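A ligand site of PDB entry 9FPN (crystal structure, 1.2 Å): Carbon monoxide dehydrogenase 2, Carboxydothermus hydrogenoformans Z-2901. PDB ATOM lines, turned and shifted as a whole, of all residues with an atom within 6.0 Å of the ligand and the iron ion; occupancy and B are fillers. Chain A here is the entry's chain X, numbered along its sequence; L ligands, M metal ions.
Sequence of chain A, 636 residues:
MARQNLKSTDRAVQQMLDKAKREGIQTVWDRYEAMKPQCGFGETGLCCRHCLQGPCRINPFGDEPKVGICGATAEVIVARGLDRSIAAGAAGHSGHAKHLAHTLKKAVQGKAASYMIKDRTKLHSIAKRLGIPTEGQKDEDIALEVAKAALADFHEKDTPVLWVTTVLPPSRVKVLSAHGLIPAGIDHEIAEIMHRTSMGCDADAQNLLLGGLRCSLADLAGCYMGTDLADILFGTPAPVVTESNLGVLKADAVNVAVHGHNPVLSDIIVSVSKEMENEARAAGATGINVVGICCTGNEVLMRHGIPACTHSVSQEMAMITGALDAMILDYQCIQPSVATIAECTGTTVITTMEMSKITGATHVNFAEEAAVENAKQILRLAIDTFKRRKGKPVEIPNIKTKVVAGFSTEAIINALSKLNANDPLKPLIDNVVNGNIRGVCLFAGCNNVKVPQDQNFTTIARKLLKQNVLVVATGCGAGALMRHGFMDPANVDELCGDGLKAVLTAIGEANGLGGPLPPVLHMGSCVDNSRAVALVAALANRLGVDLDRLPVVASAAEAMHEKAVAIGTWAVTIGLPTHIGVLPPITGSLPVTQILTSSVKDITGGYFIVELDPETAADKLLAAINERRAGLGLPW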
ATOM      1  N   HIS A  93      11.457 -13.518 -27.383  1.00  0.00           N
ATOM      2  CA  HIS A  93      11.316 -12.100 -27.058  1.00  0.00           C
ATOM      3  C   HIS A  93      12.666 -11.428 -27.006  1.00  0.00           C
ATOM      4  O   HIS A  93      12.848 -10.297 -27.467  1.00  0.00           O
ATOM      5  CB  HIS A  93      10.621 -11.892 -25.710  1.00  0.00           C
ATOM      6  CG  HIS A  93       9.171 -12.238 -25.711  1.00  0.00           C
ATOM      7  ND1 HIS A  93       8.631 -13.031 -24.745  1.00  0.00           N
ATOM      8  CD2 HIS A  93       8.137 -11.857 -26.503  1.00  0.00           C
ATOM      9  CE1 HIS A  93       7.333 -13.156 -24.951  1.00  0.00           C
ATOM     10  NE2 HIS A  93       7.007 -12.424 -25.994  1.00  0.00           N
ATOM     11  N   GLY A 260       4.372 -10.911 -38.141  1.00  0.00           N
ATOM     12  CA  GLY A 260       5.484 -11.341 -37.320  1.00  0.00           C
ATOM     13  C   GLY A 260       5.488 -10.545 -36.042  1.00  0.00           C
ATOM     14  O   GLY A 260       4.407 -10.268 -35.496  1.00  0.00           O
ATOM     15  N   HIS A 261       6.656 -10.229 -35.537  1.00  0.00           N
ATOM     16  CA  HIS A 261       6.882  -9.508 -34.277  1.00  0.00           C
ATOM     17  C   HIS A 261       7.864  -8.348 -34.349  1.00  0.00           C
ATOM     18  O   HIS A 261       7.617  -7.320 -33.706  1.00  0.00           O
ATOM     19  CB  HIS A 261       7.261 -10.533 -33.062  1.00  0.00           C
ATOM     20  CG  HIS A 261       6.051 -11.225 -32.512  1.00  0.00           C
ATOM     21  ND1 HIS A 261       5.372 -12.180 -33.226  1.00  0.00           N
ATOM     22  CD2 HIS A 261       5.343 -11.041 -31.359  1.00  0.00           C
ATOM     23  CE1 HIS A 261       4.258 -12.498 -32.583  1.00  0.00           C
ATOM     24  NE2 HIS A 261       4.179 -11.795 -31.442  1.00  0.00           N
ATOM     25  N   CYS A 294      -0.974  -9.956 -36.516  1.00  0.00           N
ATOM     26  CA  CYS A 294      -0.222 -10.258 -35.307  1.00  0.00           C
ATOM     27  C   CYS A 294       0.572  -9.050 -34.794  1.00  0.00           C
ATOM     28  O   CYS A 294       0.116  -7.913 -34.922  1.00  0.00           O
ATOM     29  CB  CYS A 294       0.603 -11.539 -35.517  1.00  0.00           C
ATOM     30  SG  CYS A 294      -0.411 -13.052 -35.600  1.00  0.00           S
ATOM     31  N   CYS A 295       1.720  -9.247 -34.265  1.00  0.00           N
ATOM     32  CA  CYS A 295       2.319  -8.175 -33.491  1.00  0.00           C
ATOM     33  C   CYS A 295       3.113  -7.186 -34.323  1.00  0.00           C
ATOM     34  O   CYS A 295       3.181  -6.018 -33.955  1.00  0.00           O
ATOM     35  CB  CYS A 295       3.131  -8.677 -32.304  1.00  0.00           C
ATOM     36  SG  CYS A 295       2.055  -9.087 -30.969  1.00  0.00           S
ATOM     37  N   ASN A 298       0.481  -5.015 -34.659  1.00  0.00           N
ATOM     38  CA  ASN A 298       0.298  -4.200 -33.461  1.00  0.00           C
ATOM     39  C   ASN A 298       1.287  -3.052 -33.412  1.00  0.00           C
ATOM     40  O   ASN A 298       0.933  -1.955 -33.022  1.00  0.00           O
ATOM     41  CB  ASN A 298       0.354  -5.014 -32.171  1.00  0.00           C
ATOM     42  CG  ASN A 298      -0.952  -5.676 -31.853  1.00  0.00           C
ATOM     43  OD1 ASN A 298      -2.011  -5.099 -31.948  1.00  0.00           O
ATOM     44  ND2 ASN A 298      -0.865  -6.924 -31.413  1.00  0.00           N
ATOM     45  N   SER A 312      -3.604 -14.048 -34.767  1.00  0.00           N
ATOM     46  CA  SER A 312      -3.022 -15.367 -34.809  1.00  0.00           C
ATOM     47  C   SER A 312      -3.803 -16.463 -35.508  1.00  0.00           C
ATOM     48  O   SER A 312      -3.460 -16.835 -36.644  1.00  0.00           O
ATOM     49  CB  SER A 312      -2.472 -15.847 -33.470  1.00  0.00           C
ATOM     50  OG  SER A 312      -3.503 -15.991 -32.516  1.00  0.00           O
ATOM     51  N   GLN A 332       8.089 -15.367 -35.750  1.00  0.00           N
ATOM     52  CA  GLN A 332       7.268 -15.769 -34.624  1.00  0.00           C
ATOM     53  C   GLN A 332       5.783 -15.691 -34.960  1.00  0.00           C
ATOM     54  O   GLN A 332       5.301 -14.637 -35.437  1.00  0.00           O
ATOM     55  CB  GLN A 332       7.499 -14.959 -33.360  1.00  0.00           C
ATOM     56  CG  GLN A 332       8.960 -14.974 -32.861  1.00  0.00           C
ATOM     57  CD  GLN A 332       9.229 -13.854 -31.877  1.00  0.00           C
ATOM     58  OE1 GLN A 332       8.304 -13.235 -31.296  1.00  0.00           O
ATOM     59  NE2 GLN A 332      10.519 -13.559 -31.671  1.00  0.00           N
ATOM     60  N   CYS A 333       5.063 -16.790 -34.716  1.00  0.00           N
ATOM     61  CA  CYS A 333       3.593 -16.856 -34.742  1.00  0.00           C
ATOM     62  C   CYS A 333       3.035 -16.873 -36.148  1.00  0.00           C
ATOM     63  O   CYS A 333       1.830 -16.747 -36.331  1.00  0.00           O
ATOM     64  CB  CYS A 333       3.009 -15.722 -33.873  1.00  0.00           C
ATOM     65  SG  CYS A 333       3.592 -15.852 -32.192  1.00  0.00           S
ATOM     66  N   ALA A 444      -3.520 -10.797 -22.322  1.00  0.00           N
ATOM     67  CA  ALA A 444      -2.297 -10.986 -23.039  1.00  0.00           C
ATOM     68  C   ALA A 444      -2.364 -12.314 -23.771  1.00  0.00           C
ATOM     69  O   ALA A 444      -3.215 -13.176 -23.504  1.00  0.00           O
ATOM     70  CB  ALA A 444      -1.095 -10.960 -22.093  1.00  0.00           C
ATOM     71  N   GLY A 445      -1.433 -12.464 -24.694  1.00  0.00           N
ATOM     72  CA  GLY A 445      -1.234 -13.716 -25.367  1.00  0.00           C
ATOM     73  C   GLY A 445      -2.233 -13.966 -26.476  1.00  0.00           C
ATOM     74  O   GLY A 445      -2.948 -13.093 -26.970  1.00  0.00           O
ATOM     75  N   CYS A 446      -2.057 -15.184 -26.979  1.00  0.00           N
ATOM     76  CA  CYS A 446      -2.620 -15.625 -28.255  1.00  0.00           C
ATOM     77  C   CYS A 446      -4.053 -16.126 -28.318  1.00  0.00           C
ATOM     78  O   CYS A 446      -4.806 -15.931 -27.320  1.00  0.00           O
ATOM     79  CB  CYS A 446      -1.743 -16.868 -28.564  1.00  0.00           C
ATOM     80  SG  CYS A 446      -0.098 -17.031 -27.748  1.00  0.00           S
ATOM     81  N   ASN A 447      -4.521 -16.416 -29.546  1.00  0.00           N
ATOM     82  CA  ASN A 447      -5.637 -17.317 -29.743  1.00  0.00           C
ATOM     83  C   ASN A 447      -5.074 -18.746 -29.836  1.00  0.00           C
ATOM     84  O   ASN A 447      -3.874 -18.937 -30.070  1.00  0.00           O
ATOM     85  CB  ASN A 447      -6.405 -17.028 -31.034  1.00  0.00           C
ATOM     86  CG  ASN A 447      -7.110 -15.645 -31.118  1.00  0.00           C
ATOM     87  OD1 ASN A 447      -6.909 -14.951 -32.103  1.00  0.00           O
ATOM     88  ND2 ASN A 447      -7.950 -15.328 -30.147  1.00  0.00           N
ATOM     89  N   THR A 474      -2.795  -6.572 -24.758  1.00  0.00           N
ATOM     90  CA  THR A 474      -1.684  -6.611 -25.696  1.00  0.00           C
ATOM     91  C   THR A 474      -1.830  -7.823 -26.625  1.00  0.00           C
ATOM     92  O   THR A 474      -2.649  -8.718 -26.413  1.00  0.00           O
ATOM     93  CB  THR A 474      -0.349  -6.765 -24.976  1.00  0.00           C
ATOM     94  OG1 THR A 474      -0.367  -8.034 -24.315  1.00  0.00           O
ATOM     95  CG2 THR A 474      -0.114  -5.647 -23.961  1.00  0.00           C
ATOM     96  N   GLY A 475      -1.028  -7.834 -27.687  1.00  0.00           N
ATOM     97  CA  GLY A 475      -0.943  -9.007 -28.549  1.00  0.00           C
ATOM     98  C   GLY A 475      -2.297  -9.405 -29.111  1.00  0.00           C
ATOM     99  O   GLY A 475      -3.102  -8.559 -29.517  1.00  0.00           O
ATOM    100  N   CYS A 476      -2.554 -10.715 -29.131  1.00  0.00           N
ATOM    101  CA  CYS A 476      -3.804 -11.238 -29.663  1.00  0.00           C
ATOM    102  C   CYS A 476      -4.976 -11.012 -28.711  1.00  0.00           C
ATOM    103  O   CYS A 476      -6.134 -11.037 -29.144  1.00  0.00           O
ATOM    104  CB  CYS A 476      -3.676 -12.724 -30.000  1.00  0.00           C
ATOM    105  SG  CYS A 476      -2.627 -13.065 -31.416  1.00  0.00           S
ATOM    106  N   GLY A 477      -4.711 -10.792 -27.425  1.00  0.00           N
ATOM    107  CA  GLY A 477      -5.762 -10.324 -26.539  1.00  0.00           C
ATOM    108  C   GLY A 477      -6.306  -8.988 -26.990  1.00  0.00           C
ATOM    109  O   GLY A 477      -7.512  -8.798 -27.142  1.00  0.00           O
ATOM    110  N   SER A 525       2.085  -4.592 -28.457  1.00  0.00           N
ATOM    111  CA  SER A 525       2.514  -5.903 -28.875  1.00  0.00           C
ATOM    112  C   SER A 525       2.846  -6.784 -27.696  1.00  0.00           C
ATOM    113  O   SER A 525       2.738  -6.413 -26.523  1.00  0.00           O
ATOM    114  CB  SER A 525       3.763  -5.783 -29.717  1.00  0.00           C
ATOM    115  OG  SER A 525       4.786  -5.227 -28.870  1.00  0.00           O
ATOM    116  N   CYS A 526       3.267  -8.003 -28.047  1.00  0.00           N
ATOM    117  CA  CYS A 526       3.640  -8.957 -26.901  1.00  0.00           C
ATOM    118  C   CYS A 526       4.886  -8.489 -26.001  1.00  0.00           C
ATOM    119  O   CYS A 526       4.932  -8.601 -24.708  1.00  0.00           O
ATOM    120  CB  CYS A 526       3.843 -10.411 -27.433  1.00  0.00           C
ATOM    121  SG  CYS A 526       2.263 -11.072 -28.042  1.00  0.00           S
ATOM    122  N   MET A 560      -1.174 -19.907 -26.431  1.00  0.00           N
ATOM    123  CA  MET A 560      -0.645 -20.837 -27.412  1.00  0.00           C
ATOM    124  C   MET A 560       0.892 -20.928 -27.370  1.00  0.00           C
ATOM    125  O   MET A 560       1.458 -22.018 -27.233  1.00  0.00           O
ATOM    126  CB  MET A 560      -1.132 -20.484 -28.821  1.00  0.00           C
ATOM    127  CG  MET A 560      -0.666 -21.409 -29.909  1.00  0.00           C
ATOM    128  SD  MET A 560       0.877 -20.875 -30.759  1.00  0.00           S
ATOM    129  CE  MET A 560       0.435 -19.288 -31.407  1.00  0.00           C
ATOM    130  N   HIS A 561       1.583 -19.825 -27.568  1.00  0.00           N
ATOM    131  CA  HIS A 561       3.003 -19.877 -27.875  1.00  0.00           C
ATOM    132  C   HIS A 561       3.857 -20.064 -26.605  1.00  0.00           C
ATOM    133  O   HIS A 561       3.445 -19.677 -25.512  1.00  0.00           O
ATOM    134  CB  HIS A 561       3.394 -18.560 -28.558  1.00  0.00           C
ATOM    135  CG  HIS A 561       4.642 -18.636 -29.359  1.00  0.00           C
ATOM    136  ND1 HIS A 561       5.921 -18.539 -28.785  1.00  0.00           N
ATOM    137  CD2 HIS A 561       4.832 -18.814 -30.677  1.00  0.00           C
ATOM    138  CE1 HIS A 561       6.828 -18.676 -29.739  1.00  0.00           C
ATOM    139  NE2 HIS A 561       6.204 -18.849 -30.903  1.00  0.00           N
ATOM    140  N   LYS A 563       6.188 -18.256 -25.955  1.00  0.00           N
ATOM    141  CA  LYS A 563       6.286 -16.894 -25.446  1.00  0.00           C
ATOM    142  C   LYS A 563       5.199 -16.549 -24.434  1.00  0.00           C
ATOM    143  O   LYS A 563       5.454 -15.793 -23.476  1.00  0.00           O
ATOM    144  CB  LYS A 563       6.199 -15.923 -26.612  1.00  0.00           C
ATOM    145  CG  LYS A 563       7.488 -15.789 -27.427  1.00  0.00           C
ATOM    146  CD  LYS A 563       7.336 -14.827 -28.601  1.00  0.00           C
ATOM    147  CE  LYS A 563       6.466 -15.333 -29.691  1.00  0.00           C
ATOM    148  NZ  LYS A 563       5.867 -14.228 -30.509  1.00  0.00           N
ATOM    149  N   ALA A 564       3.986 -17.034 -24.653  1.00  0.00           N
ATOM    150  CA  ALA A 564       2.891 -16.778 -23.725  1.00  0.00           C
ATOM    151  C   ALA A 564       3.065 -17.513 -22.395  1.00  0.00           C
ATOM    152  O   ALA A 564       2.734 -16.966 -21.320  1.00  0.00           O
ATOM    153  CB  ALA A 564       1.560 -17.110 -24.402  1.00  0.00           C
ATOM    154  N   ILE A 567       5.579 -15.318 -20.541  1.00  0.00           N
ATOM    155  CA  ILE A 567       4.934 -14.116 -20.005  1.00  0.00           C
ATOM    156  C   ILE A 567       4.090 -14.483 -18.802  1.00  0.00           C
ATOM    157  O   ILE A 567       4.112 -13.798 -17.784  1.00  0.00           O
ATOM    158  CB  ILE A 567       4.101 -13.460 -21.102  1.00  0.00           C
ATOM    159  CG1 ILE A 567       4.983 -12.785 -22.158  1.00  0.00           C
ATOM    160  CG2 ILE A 567       3.113 -12.424 -20.482  1.00  0.00           C
ATOM    161  CD1 ILE A 567       4.298 -12.524 -23.489  1.00  0.00           C
HETATM  162 NI1  LIG L   1       2.058 -13.107 -28.574  1.00  0.00          NI
HETATM  163 FE1  LIG L   1       2.009 -14.637 -31.118  1.00  0.00          FE
HETATM  164 FE2  LIG L   1       0.674 -15.229 -29.046  1.00  0.00          FE
HETATM  165 FE3  LIG L   1      -0.423 -13.555 -30.865  1.00  0.00          FE
HETATM  166  S1  LIG L   1      -0.113 -13.115 -28.665  1.00  0.00           S
HETATM  167  S2  LIG L   1      -0.031 -15.792 -31.209  1.00  0.00           S
HETATM  168  S3  LIG L   1       1.273 -12.655 -32.064  1.00  0.00           S
HETATM  169  S4  LIG L   1       2.904 -15.019 -28.945  1.00  0.00           S
HETATM  170 FE    FE M   1       2.432 -11.389 -30.489  1.00  0.00          FE
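O of Gly 445 sits close to S1 of the ligand, at 3.3 Å.
Cys 294 touches the ligand (CB to S3, 3.7 Å).
Met 560 touches the ligand.
His 561 touches the ligand.
Within 4 Å of the ligand: His 261, Cys 294, Cys 295, Ser 312, Cys 333, Gly 445, Cys 446, Cys 476, Cys 526, Met 560, His 561 and Lys 563.
Three residues have an atom within 4 Å of the iron ion: His 261, Cys 295 and Cys 526.
The nearest printed residue that does not touch the iron ion is Lys 563 (4.5 Å).
The backbone carbonyl oxygen (O) of Gly 445 sits close to the backbone NH (N) of Cys 476.
O of Gly 260 lies within hydrogen-bond range of N of Cys 295.
A ring nitrogen (ND1) of His 561 is in hydrogen-bond range of the backbone NH (N) of Lys 563, 2.9 Å away.
N of Gly 477 lies within hydrogen-bond range of O of Gly 445.
The backbone NH of Ser 312 lies within hydrogen-bond range of the side-chain sulfur of Cys 294, at 3.4 Å.
SG of Cys 295 sits close to ND2 of Asn 298 (3.7 Å).
The side-chain sulfur (SG) of Cys 476 lies close to the side-chain hydroxyl (OG) of Ser 312, at 3.2 Å.
NZ of Lys 563 sits close to ND1 of His 261, 3.4 Å away.
The iron ion is bound by NE2 of His 261 (2.0 Å), S3 of the ligand (2.3 Å), SG of Cys 295 (2.4 Å) and SG of Cys 526 (2.5 Å).
The iron ion has four donor atoms within binding distance.
SG of Cys 476 binds FE3 of the ligand, at 2.3 Å.
The side-chain sulfur (SG) of Cys 526 is bound to a nickel atom (NI1) of the ligand.
The side-chain sulfur (SG) of Cys 446 is bound to an iron atom (FE2) of the ligand, at 2.4 Å.
A sulfur (S4) of the ligand sits close to the side-chain amino group of Lys 563 (3.4 Å).
A sulfur (S2) of the ligand sits close to the side-chain hydroxyl (OG) of Ser 312 (3.7 Å).
The backbone NH of Cys 476 lies close to a sulfur (S1) of the ligand (3.5 Å).
SG of Cys 333 binds FE1 of the ligand (2.3 Å).
The backbone NH (N) of Cys 446 sits close to a sulfur (S1) of the ligand, 3.3 Å away.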
